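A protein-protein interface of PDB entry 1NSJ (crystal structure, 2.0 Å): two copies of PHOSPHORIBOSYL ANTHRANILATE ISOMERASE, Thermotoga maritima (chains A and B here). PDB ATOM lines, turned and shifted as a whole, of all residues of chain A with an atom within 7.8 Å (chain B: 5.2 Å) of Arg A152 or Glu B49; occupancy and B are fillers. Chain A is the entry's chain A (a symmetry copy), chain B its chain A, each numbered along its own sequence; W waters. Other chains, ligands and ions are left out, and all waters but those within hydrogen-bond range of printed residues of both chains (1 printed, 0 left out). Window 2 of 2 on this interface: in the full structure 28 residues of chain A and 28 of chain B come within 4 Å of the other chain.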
ATOM      1  N   LEU A  99     -21.723 -35.435 -24.815  1.00  0.00           N
ATOM      2  CA  LEU A  99     -21.659 -33.972 -24.879  1.00  0.00           C
ATOM      3  C   LEU A  99     -20.254 -33.441 -25.288  1.00  0.00           C
ATOM      4  O   LEU A  99     -19.208 -33.913 -24.780  1.00  0.00           O
ATOM      5  CB  LEU A  99     -22.090 -33.391 -23.521  1.00  0.00           C
ATOM      6  CG  LEU A  99     -22.349 -31.899 -23.308  1.00  0.00           C
ATOM      7  CD1 LEU A  99     -23.226 -31.729 -22.107  1.00  0.00           C
ATOM      8  CD2 LEU A  99     -21.056 -31.146 -23.107  1.00  0.00           C
ATOM      9  N   TYR A 118     -19.159 -22.306 -34.330  1.00  0.00           N
ATOM     10  CA  TYR A 118     -19.320 -23.438 -33.445  1.00  0.00           C
ATOM     11  C   TYR A 118     -20.373 -23.175 -32.371  1.00  0.00           C
ATOM     12  O   TYR A 118     -20.589 -24.016 -31.503  1.00  0.00           O
ATOM     13  CB  TYR A 118     -17.978 -23.748 -32.776  1.00  0.00           C
ATOM     14  CG  TYR A 118     -16.923 -24.290 -33.703  1.00  0.00           C
ATOM     15  CD1 TYR A 118     -16.879 -25.648 -34.027  1.00  0.00           C
ATOM     16  CD2 TYR A 118     -15.962 -23.453 -34.257  1.00  0.00           C
ATOM     17  CE1 TYR A 118     -15.901 -26.157 -34.862  1.00  0.00           C
ATOM     18  CE2 TYR A 118     -14.982 -23.953 -35.095  1.00  0.00           C
ATOM     19  CZ  TYR A 118     -14.958 -25.303 -35.397  1.00  0.00           C
ATOM     20  OH  TYR A 118     -13.967 -25.791 -36.216  1.00  0.00           O
ATOM     21  N   ARG A 119     -21.078 -22.055 -32.475  1.00  0.00           N
ATOM     22  CA  ARG A 119     -22.071 -21.667 -31.472  1.00  0.00           C
ATOM     23  C   ARG A 119     -23.158 -22.664 -31.087  1.00  0.00           C
ATOM     24  O   ARG A 119     -23.865 -22.437 -30.110  1.00  0.00           O
ATOM     25  CB  ARG A 119     -22.703 -20.302 -31.792  1.00  0.00           C
ATOM     26  CG  ARG A 119     -23.310 -20.166 -33.179  1.00  0.00           C
ATOM     27  CD  ARG A 119     -23.765 -18.735 -33.454  1.00  0.00           C
ATOM     28  NE  ARG A 119     -24.943 -18.445 -32.654  1.00  0.00           N
ATOM     29  CZ  ARG A 119     -26.168 -18.287 -33.146  1.00  0.00           C
ATOM     30  NH1 ARG A 119     -26.373 -18.324 -34.460  1.00  0.00           N
ATOM     31  NH2 ARG A 119     -27.183 -18.040 -32.322  1.00  0.00           N
ATOM     32  N   GLU A 120     -23.306 -23.749 -31.839  1.00  0.00           N
ATOM     33  CA  GLU A 120     -24.319 -24.743 -31.499  1.00  0.00           C
ATOM     34  C   GLU A 120     -23.861 -25.608 -30.301  1.00  0.00           C
ATOM     35  O   GLU A 120     -24.683 -26.246 -29.631  1.00  0.00           O
ATOM     36  CB  GLU A 120     -24.691 -25.603 -32.720  1.00  0.00           C
ATOM     37  CG  GLU A 120     -23.662 -26.652 -33.142  1.00  0.00           C
ATOM     38  CD  GLU A 120     -23.984 -27.284 -34.490  1.00  0.00           C
ATOM     39  OE1 GLU A 120     -23.522 -26.745 -35.519  1.00  0.00           O
ATOM     40  OE2 GLU A 120     -24.695 -28.315 -34.522  1.00  0.00           O
ATOM     41  N   PHE A 121     -22.558 -25.575 -30.017  1.00  0.00           N
ATOM     42  CA  PHE A 121     -21.950 -26.316 -28.915  1.00  0.00           C
ATOM     43  C   PHE A 121     -21.504 -25.378 -27.793  1.00  0.00           C
ATOM     44  O   PHE A 121     -21.365 -24.168 -27.996  1.00  0.00           O
ATOM     45  CB  PHE A 121     -20.670 -27.031 -29.393  1.00  0.00           C
ATOM     46  CG  PHE A 121     -20.884 -27.976 -30.521  1.00  0.00           C
ATOM     47  CD1 PHE A 121     -21.492 -29.209 -30.312  1.00  0.00           C
ATOM     48  CD2 PHE A 121     -20.471 -27.644 -31.799  1.00  0.00           C
ATOM     49  CE1 PHE A 121     -21.692 -30.090 -31.373  1.00  0.00           C
ATOM     50  CE2 PHE A 121     -20.664 -28.514 -32.860  1.00  0.00           C
ATOM     51  CZ  PHE A 121     -21.273 -29.737 -32.649  1.00  0.00           C
ATOM     52  N   PRO A 122     -21.349 -25.915 -26.566  1.00  0.00           N
ATOM     53  CA  PRO A 122     -20.879 -25.061 -25.472  1.00  0.00           C
ATOM     54  C   PRO A 122     -19.454 -24.711 -25.964  1.00  0.00           C
ATOM     55  O   PRO A 122     -18.756 -25.580 -26.517  1.00  0.00           O
ATOM     56  CB  PRO A 122     -20.786 -26.040 -24.296  1.00  0.00           C
ATOM     57  CG  PRO A 122     -21.834 -27.048 -24.598  1.00  0.00           C
ATOM     58  CD  PRO A 122     -21.726 -27.253 -26.077  1.00  0.00           C
ATOM     59  N   ILE A 123     -19.005 -23.480 -25.753  1.00  0.00           N
ATOM     60  CA  ILE A 123     -17.697 -23.090 -26.242  1.00  0.00           C
ATOM     61  C   ILE A 123     -16.775 -22.787 -25.106  1.00  0.00           C
ATOM     62  O   ILE A 123     -17.192 -22.164 -24.141  1.00  0.00           O
ATOM     63  CB  ILE A 123     -17.794 -21.780 -27.102  1.00  0.00           C
ATOM     64  CG1 ILE A 123     -18.613 -22.031 -28.358  1.00  0.00           C
ATOM     65  CG2 ILE A 123     -16.403 -21.300 -27.550  1.00  0.00           C
ATOM     66  CD1 ILE A 123     -17.921 -22.931 -29.326  1.00  0.00           C
ATOM     67  N   TYR A 147     -20.007 -10.444 -28.042  1.00  0.00           N
ATOM     68  CA  TYR A 147     -20.371 -11.725 -28.631  1.00  0.00           C
ATOM     69  C   TYR A 147     -21.043 -12.652 -27.636  1.00  0.00           C
ATOM     70  O   TYR A 147     -21.562 -13.698 -28.032  1.00  0.00           O
ATOM     71  CB  TYR A 147     -19.135 -12.451 -29.127  1.00  0.00           C
ATOM     72  CG  TYR A 147     -18.380 -11.715 -30.183  1.00  0.00           C
ATOM     73  CD1 TYR A 147     -18.702 -11.876 -31.524  1.00  0.00           C
ATOM     74  CD2 TYR A 147     -17.323 -10.887 -29.847  1.00  0.00           C
ATOM     75  CE1 TYR A 147     -17.992 -11.235 -32.498  1.00  0.00           C
ATOM     76  CE2 TYR A 147     -16.607 -10.240 -30.812  1.00  0.00           C
ATOM     77  CZ  TYR A 147     -16.948 -10.422 -32.136  1.00  0.00           C
ATOM     78  OH  TYR A 147     -16.251  -9.760 -33.106  1.00  0.00           O
ATOM     79  N   ARG A 148     -20.995 -12.291 -26.352  1.00  0.00           N
ATOM     80  CA  ARG A 148     -21.551 -13.136 -25.293  1.00  0.00           C
ATOM     81  C   ARG A 148     -22.912 -13.792 -25.534  1.00  0.00           C
ATOM     82  O   ARG A 148     -23.009 -15.021 -25.482  1.00  0.00           O
ATOM     83  CB  ARG A 148     -21.575 -12.429 -23.945  1.00  0.00           C
ATOM     84  CG  ARG A 148     -21.874 -13.394 -22.787  1.00  0.00           C
ATOM     85  CD  ARG A 148     -22.629 -12.702 -21.693  1.00  0.00           C
ATOM     86  NE  ARG A 148     -22.998 -13.602 -20.610  1.00  0.00           N
ATOM     87  CZ  ARG A 148     -24.154 -14.257 -20.540  1.00  0.00           C
ATOM     88  NH1 ARG A 148     -25.045 -14.165 -21.514  1.00  0.00           N
ATOM     89  NH2 ARG A 148     -24.413 -15.036 -19.500  1.00  0.00           N
ATOM     90  N   ASP A 149     -23.946 -13.016 -25.835  1.00  0.00           N
ATOM     91  CA  ASP A 149     -25.271 -13.596 -26.045  1.00  0.00           C
ATOM     92  C   ASP A 149     -25.484 -14.397 -27.349  1.00  0.00           C
ATOM     93  O   ASP A 149     -26.583 -14.898 -27.604  1.00  0.00           O
ATOM     94  CB  ASP A 149     -26.352 -12.528 -25.825  1.00  0.00           C
ATOM     95  CG  ASP A 149     -26.277 -11.904 -24.427  1.00  0.00           C
ATOM     96  OD1 ASP A 149     -25.813 -12.577 -23.487  1.00  0.00           O
ATOM     97  OD2 ASP A 149     -26.669 -10.731 -24.265  1.00  0.00           O
ATOM     98  N   ARG A 150     -24.439 -14.534 -28.163  1.00  0.00           N
ATOM     99  CA  ARG A 150     -24.523 -15.324 -29.391  1.00  0.00           C
ATOM    100  C   ARG A 150     -24.334 -16.824 -29.080  1.00  0.00           C
ATOM    101  O   ARG A 150     -24.741 -17.689 -29.856  1.00  0.00           O
ATOM    102  CB  ARG A 150     -23.457 -14.879 -30.398  1.00  0.00           C
ATOM    103  CG  ARG A 150     -23.522 -13.423 -30.757  1.00  0.00           C
ATOM    104  CD  ARG A 150     -24.868 -13.095 -31.336  1.00  0.00           C
ATOM    105  NE  ARG A 150     -25.115 -13.888 -32.527  1.00  0.00           N
ATOM    106  CZ  ARG A 150     -26.314 -14.317 -32.907  1.00  0.00           C
ATOM    107  NH1 ARG A 150     -27.388 -14.050 -32.174  1.00  0.00           N
ATOM    108  NH2 ARG A 150     -26.439 -15.030 -34.015  1.00  0.00           N
ATOM    109  N   PHE A 151     -23.684 -17.116 -27.955  1.00  0.00           N
ATOM    110  CA  PHE A 151     -23.409 -18.488 -27.524  1.00  0.00           C
ATOM    111  C   PHE A 151     -24.405 -18.988 -26.459  1.00  0.00           C
ATOM    112  O   PHE A 151     -24.965 -18.200 -25.699  1.00  0.00           O
ATOM    113  CB  PHE A 151     -21.976 -18.571 -26.976  1.00  0.00           C
ATOM    114  CG  PHE A 151     -20.929 -18.162 -27.965  1.00  0.00           C
ATOM    115  CD1 PHE A 151     -20.514 -19.040 -28.968  1.00  0.00           C
ATOM    116  CD2 PHE A 151     -20.384 -16.883 -27.924  1.00  0.00           C
ATOM    117  CE1 PHE A 151     -19.577 -18.649 -29.915  1.00  0.00           C
ATOM    118  CE2 PHE A 151     -19.448 -16.483 -28.864  1.00  0.00           C
ATOM    119  CZ  PHE A 151     -19.042 -17.366 -29.864  1.00  0.00           C
ATOM    120  N   ARG A 152     -24.621 -20.296 -26.397  1.00  0.00           N
ATOM    121  CA  ARG A 152     -25.528 -20.859 -25.394  1.00  0.00           C
ATOM    122  C   ARG A 152     -24.835 -20.834 -24.026  1.00  0.00           C
ATOM    123  O   ARG A 152     -25.336 -20.243 -23.072  1.00  0.00           O
ATOM    124  CB  ARG A 152     -25.860 -22.311 -25.733  1.00  0.00           C
ATOM    125  CG  ARG A 152     -26.275 -22.601 -27.163  1.00  0.00           C
ATOM    126  CD  ARG A 152     -26.038 -24.087 -27.433  1.00  0.00           C
ATOM    127  NE  ARG A 152     -27.219 -24.792 -27.929  1.00  0.00           N
ATOM    128  CZ  ARG A 152     -28.258 -25.182 -27.184  1.00  0.00           C
ATOM    129  NH1 ARG A 152     -28.307 -24.947 -25.874  1.00  0.00           N
ATOM    130  NH2 ARG A 152     -29.259 -25.832 -27.765  1.00  0.00           N
ATOM    131  N   TYR A 153     -23.686 -21.506 -23.944  1.00  0.00           N
ATOM    132  CA  TYR A 153     -22.925 -21.592 -22.705  1.00  0.00           C
ATOM    133  C   TYR A 153     -21.468 -21.339 -23.011  1.00  0.00           C
ATOM    134  O   TYR A 153     -20.917 -21.897 -23.959  1.00  0.00           O
ATOM    135  CB  TYR A 153     -23.100 -22.967 -22.043  1.00  0.00           C
ATOM    136  CG  TYR A 153     -24.537 -23.292 -21.704  1.00  0.00           C
ATOM    137  CD1 TYR A 153     -25.178 -22.669 -20.636  1.00  0.00           C
ATOM    138  CD2 TYR A 153     -25.270 -24.192 -22.483  1.00  0.00           C
ATOM    139  CE1 TYR A 153     -26.516 -22.931 -20.352  1.00  0.00           C
ATOM    140  CE2 TYR A 153     -26.605 -24.464 -22.209  1.00  0.00           C
ATOM    141  CZ  TYR A 153     -27.224 -23.824 -21.144  1.00  0.00           C
ATOM    142  OH  TYR A 153     -28.562 -24.055 -20.888  1.00  0.00           O
ATOM    143  N   LEU A 154     -20.847 -20.519 -22.177  1.00  0.00           N
ATOM    144  CA  LEU A 154     -19.463 -20.132 -22.355  1.00  0.00           C
ATOM    145  C   LEU A 154     -18.598 -20.471 -21.154  1.00  0.00           C
ATOM    146  O   LEU A 154     -18.951 -20.177 -20.011  1.00  0.00           O
ATOM    147  CB  LEU A 154     -19.433 -18.615 -22.569  1.00  0.00           C
ATOM    148  CG  LEU A 154     -18.624 -17.901 -23.638  1.00  0.00           C
ATOM    149  CD1 LEU A 154     -18.626 -18.673 -24.945  1.00  0.00           C
ATOM    150  CD2 LEU A 154     -19.253 -16.526 -23.819  1.00  0.00           C
ATOM    151  N   PHE A 175     -20.675 -19.064 -18.031  1.00  0.00           N
ATOM    152  CA  PHE A 175     -21.357 -20.154 -17.330  1.00  0.00           C
ATOM    153  C   PHE A 175     -20.329 -20.806 -16.424  1.00  0.00           C
ATOM    154  O   PHE A 175     -20.595 -21.116 -15.265  1.00  0.00           O
ATOM    155  CB  PHE A 175     -21.883 -21.203 -18.313  1.00  0.00           C
ATOM    156  CG  PHE A 175     -22.418 -22.448 -17.648  1.00  0.00           C
ATOM    157  CD1 PHE A 175     -23.634 -22.421 -16.966  1.00  0.00           C
ATOM    158  CD2 PHE A 175     -21.709 -23.646 -17.703  1.00  0.00           C
ATOM    159  CE1 PHE A 175     -24.141 -23.579 -16.351  1.00  0.00           C
ATOM    160  CE2 PHE A 175     -22.208 -24.804 -17.092  1.00  0.00           C
ATOM    161  CZ  PHE A 175     -23.424 -24.771 -16.415  1.00  0.00           C
ATOM    162  N   LEU B  12     -38.388 -28.599 -19.705  1.00  0.00           N
ATOM    163  CA  LEU B  12     -37.202 -27.776 -19.922  1.00  0.00           C
ATOM    164  C   LEU B  12     -37.064 -26.558 -19.024  1.00  0.00           C
ATOM    165  O   LEU B  12     -35.998 -26.374 -18.429  1.00  0.00           O
ATOM    166  CB  LEU B  12     -37.080 -27.373 -21.405  1.00  0.00           C
ATOM    167  CG  LEU B  12     -35.842 -26.594 -21.877  1.00  0.00           C
ATOM    168  CD1 LEU B  12     -34.607 -27.467 -21.765  1.00  0.00           C
ATOM    169  CD2 LEU B  12     -36.046 -26.100 -23.304  1.00  0.00           C
ATOM    170  N   LEU B  16     -33.868 -25.770 -16.575  1.00  0.00           N
ATOM    171  CA  LEU B  16     -32.979 -24.618 -16.735  1.00  0.00           C
ATOM    172  C   LEU B  16     -32.987 -23.709 -15.509  1.00  0.00           C
ATOM    173  O   LEU B  16     -31.957 -23.163 -15.121  1.00  0.00           O
ATOM    174  CB  LEU B  16     -33.323 -23.825 -18.007  1.00  0.00           C
ATOM    175  CG  LEU B  16     -33.078 -24.544 -19.326  1.00  0.00           C
ATOM    176  CD1 LEU B  16     -33.681 -23.713 -20.447  1.00  0.00           C
ATOM    177  CD2 LEU B  16     -31.576 -24.834 -19.522  1.00  0.00           C
ATOM    178  N   ARG B  44     -34.549 -36.856 -23.539  1.00  0.00           N
ATOM    179  CA  ARG B  44     -33.422 -36.580 -24.421  1.00  0.00           C
ATOM    180  C   ARG B  44     -33.403 -35.109 -24.882  1.00  0.00           C
ATOM    181  O   ARG B  44     -32.353 -34.484 -24.888  1.00  0.00           O
ATOM    182  CB  ARG B  44     -33.418 -37.532 -25.625  1.00  0.00           C
ATOM    183  CG  ARG B  44     -32.169 -37.363 -26.477  1.00  0.00           C
ATOM    184  CD  ARG B  44     -32.127 -38.242 -27.722  1.00  0.00           C
ATOM    185  NE  ARG B  44     -30.746 -38.351 -28.199  1.00  0.00           N
ATOM    186  CZ  ARG B  44     -30.151 -37.474 -29.009  1.00  0.00           C
ATOM    187  NH1 ARG B  44     -30.812 -36.414 -29.462  1.00  0.00           N
ATOM    188  NH2 ARG B  44     -28.866 -37.618 -29.312  1.00  0.00           N
ATOM    189  N   ARG B  45     -34.573 -34.565 -25.222  1.00  0.00           N
ATOM    190  CA  ARG B  45     -34.729 -33.162 -25.671  1.00  0.00           C
ATOM    191  C   ARG B  45     -34.182 -32.187 -24.652  1.00  0.00           C
ATOM    192  O   ARG B  45     -33.537 -31.190 -24.992  1.00  0.00           O
ATOM    193  CB  ARG B  45     -36.204 -32.784 -25.837  1.00  0.00           C
ATOM    194  CG  ARG B  45     -36.860 -33.356 -27.025  1.00  0.00           C
ATOM    195  CD  ARG B  45     -38.290 -32.827 -27.276  1.00  0.00           C
ATOM    196  NE  ARG B  45     -38.727 -33.295 -28.587  1.00  0.00           N
ATOM    197  CZ  ARG B  45     -39.547 -34.343 -28.788  1.00  0.00           C
ATOM    198  NH1 ARG B  45     -40.030 -35.071 -27.737  1.00  0.00           N
ATOM    199  NH2 ARG B  45     -39.887 -34.715 -30.035  1.00  0.00           N
ATOM    200  N   ILE B  46     -34.504 -32.462 -23.395  1.00  0.00           N
ATOM    201  CA  ILE B  46     -34.078 -31.639 -22.284  1.00  0.00           C
ATOM    202  C   ILE B  46     -32.593 -31.797 -21.995  1.00  0.00           C
ATOM    203  O   ILE B  46     -31.884 -30.804 -21.840  1.00  0.00           O
ATOM    204  CB  ILE B  46     -34.875 -31.987 -21.042  1.00  0.00           C
ATOM    205  CG1 ILE B  46     -36.370 -31.710 -21.272  1.00  0.00           C
ATOM    206  CG2 ILE B  46     -34.333 -31.218 -19.876  1.00  0.00           C
ATOM    207  CD1 ILE B  46     -37.289 -32.102 -20.102  1.00  0.00           C
ATOM    208  N   SER B  47     -32.118 -33.038 -21.961  1.00  0.00           N
ATOM    209  CA  SER B  47     -30.713 -33.319 -21.666  1.00  0.00           C
ATOM    210  C   SER B  47     -29.754 -32.610 -22.638  1.00  0.00           C
ATOM    211  O   SER B  47     -28.746 -32.014 -22.256  1.00  0.00           O
ATOM    212  CB  SER B  47     -30.481 -34.831 -21.732  1.00  0.00           C
ATOM    213  OG  SER B  47     -29.152 -35.169 -21.379  1.00  0.00           O
ATOM    214  N   VAL B  48     -30.078 -32.724 -23.913  1.00  0.00           N
ATOM    215  CA  VAL B  48     -29.290 -32.154 -24.986  1.00  0.00           C
ATOM    216  C   VAL B  48     -29.180 -30.614 -24.915  1.00  0.00           C
ATOM    217  O   VAL B  48     -28.165 -30.042 -25.279  1.00  0.00           O
ATOM    218  CB  VAL B  48     -29.866 -32.704 -26.320  1.00  0.00           C
ATOM    219  CG1 VAL B  48     -30.185 -31.614 -27.287  1.00  0.00           C
ATOM    220  CG2 VAL B  48     -28.934 -33.764 -26.881  1.00  0.00           C
ATOM    221  N   GLU B  49     -30.186 -29.976 -24.336  1.00  0.00           N
ATOM    222  CA  GLU B  49     -30.280 -28.526 -24.186  1.00  0.00           C
ATOM    223  C   GLU B  49     -29.529 -27.958 -22.959  1.00  0.00           C
ATOM    224  O   GLU B  49     -29.196 -26.759 -22.899  1.00  0.00           O
ATOM    225  CB  GLU B  49     -31.764 -28.198 -24.045  1.00  0.00           C
ATOM    226  CG  GLU B  49     -32.178 -26.855 -24.518  1.00  0.00           C
ATOM    227  CD  GLU B  49     -31.949 -26.681 -25.997  1.00  0.00           C
ATOM    228  OE1 GLU B  49     -32.042 -27.674 -26.756  1.00  0.00           O
ATOM    229  OE2 GLU B  49     -31.665 -25.534 -26.396  1.00  0.00           O
ATOM    230  N   LEU B  50     -29.328 -28.807 -21.954  1.00  0.00           N
ATOM    231  CA  LEU B  50     -28.670 -28.425 -20.704  1.00  0.00           C
ATOM    232  C   LEU B  50     -27.178 -28.197 -20.879  1.00  0.00           C
ATOM    233  O   LEU B  50     -26.555 -28.805 -21.732  1.00  0.00           O
ATOM    234  CB  LEU B  50     -28.899 -29.514 -19.648  1.00  0.00           C
ATOM    235  CG  LEU B  50     -30.339 -29.770 -19.190  1.00  0.00           C
ATOM    236  CD1 LEU B  50     -30.380 -30.934 -18.195  1.00  0.00           C
ATOM    237  CD2 LEU B  50     -30.901 -28.510 -18.562  1.00  0.00           C
ATOM    238  N   PRO B  51     -26.582 -27.332 -20.047  1.00  0.00           N
ATOM    239  CA  PRO B  51     -25.147 -27.063 -20.148  1.00  0.00           C
ATOM    240  C   PRO B  51     -24.289 -28.187 -19.588  1.00  0.00           C
ATOM    241  O   PRO B  51     -24.794 -29.138 -18.977  1.00  0.00           O
ATOM    242  CB  PRO B  51     -24.991 -25.844 -19.252  1.00  0.00           C
ATOM    243  CG  PRO B  51     -26.000 -26.108 -18.182  1.00  0.00           C
ATOM    244  CD  PRO B  51     -27.190 -26.516 -18.991  1.00  0.00           C
HETATM  245  O   HOH W   1     -30.336 -24.137 -23.600  1.00  0.00           O
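O of Glu A120 lies close to NE of Arg A152, 3.4 Å away. N of Ile A123 is in hydrogen-bond range of O of Tyr A153 (3.1 Å). O of Leu A154 lies within hydrogen-bond range of N of Phe A175 (2.9 Å).
Hydrophobic or aromatic side chains of chain A within 4 Å of the printed part of chain B: Tyr A153 and Phe A175. Of the 10 printed residues of chain B, 3 touch a printed residue of chain A. Printed residues of chain B that touch a printed residue of chain A: Leu B16, Glu B49 and Pro B51. Hydrophobic or aromatic side chains of chain B within 4 Å of the printed part of chain A: Leu B16 and Pro B51. Along chain B the printed residues that touch a printed residue of chain A span positions 16 to 51. Among the printed residues, Asp or Glu carboxylates within 4 Å of a Lys or Arg side-chain nitrogen of the other chain: Arg A152 with Glu B49 (2.8 Å).
Water W1 lies within hydrogen-bond range of the backbone carbonyl oxygen of Glu B49, the guanidinium group of Arg A152 and the side-chain hydroxyl of Tyr A153.
Among the printed residues, pairs that only touch across the chains: Tyr A153 with Pro B51, Phe A175 with Pro B51 and Tyr A153 with Leu B16.
Of chain B, only Glu B49 (2.8 Å) comes within 4 Å of Arg A152. Of the printed residues of chain A, Glu B49 touches Arg A152 (2.8 Å) and Tyr A153 (3.4 Å). Of the printed residues of chain A, Leu B16 touches Tyr A153 (3.4 Å). Of the printed residues of chain B, Phe A175 touches Pro B51. Tyr A147 touches none of the printed residues of chain B. The nearest residue of chain A that does not touch Glu B49 is Leu A99 (7.4 Å). The nearest printed residue of chain B that does not touch Tyr A153 is Leu B50 (4.004 Å).
No position is printed for both chains. Of the 5 pairs that touch across the chains among the printed residues, none has its exchanged pair printed and touching as well.
The guanidinium group (NH2) of Arg A152 is in salt-bridge range of the side-chain carboxylate (OE2) of Glu B49, at 2.8 Å. O of Glu B49 sits at hydrogen-bond distance from OH of Tyr A153, 3.4 Å away.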
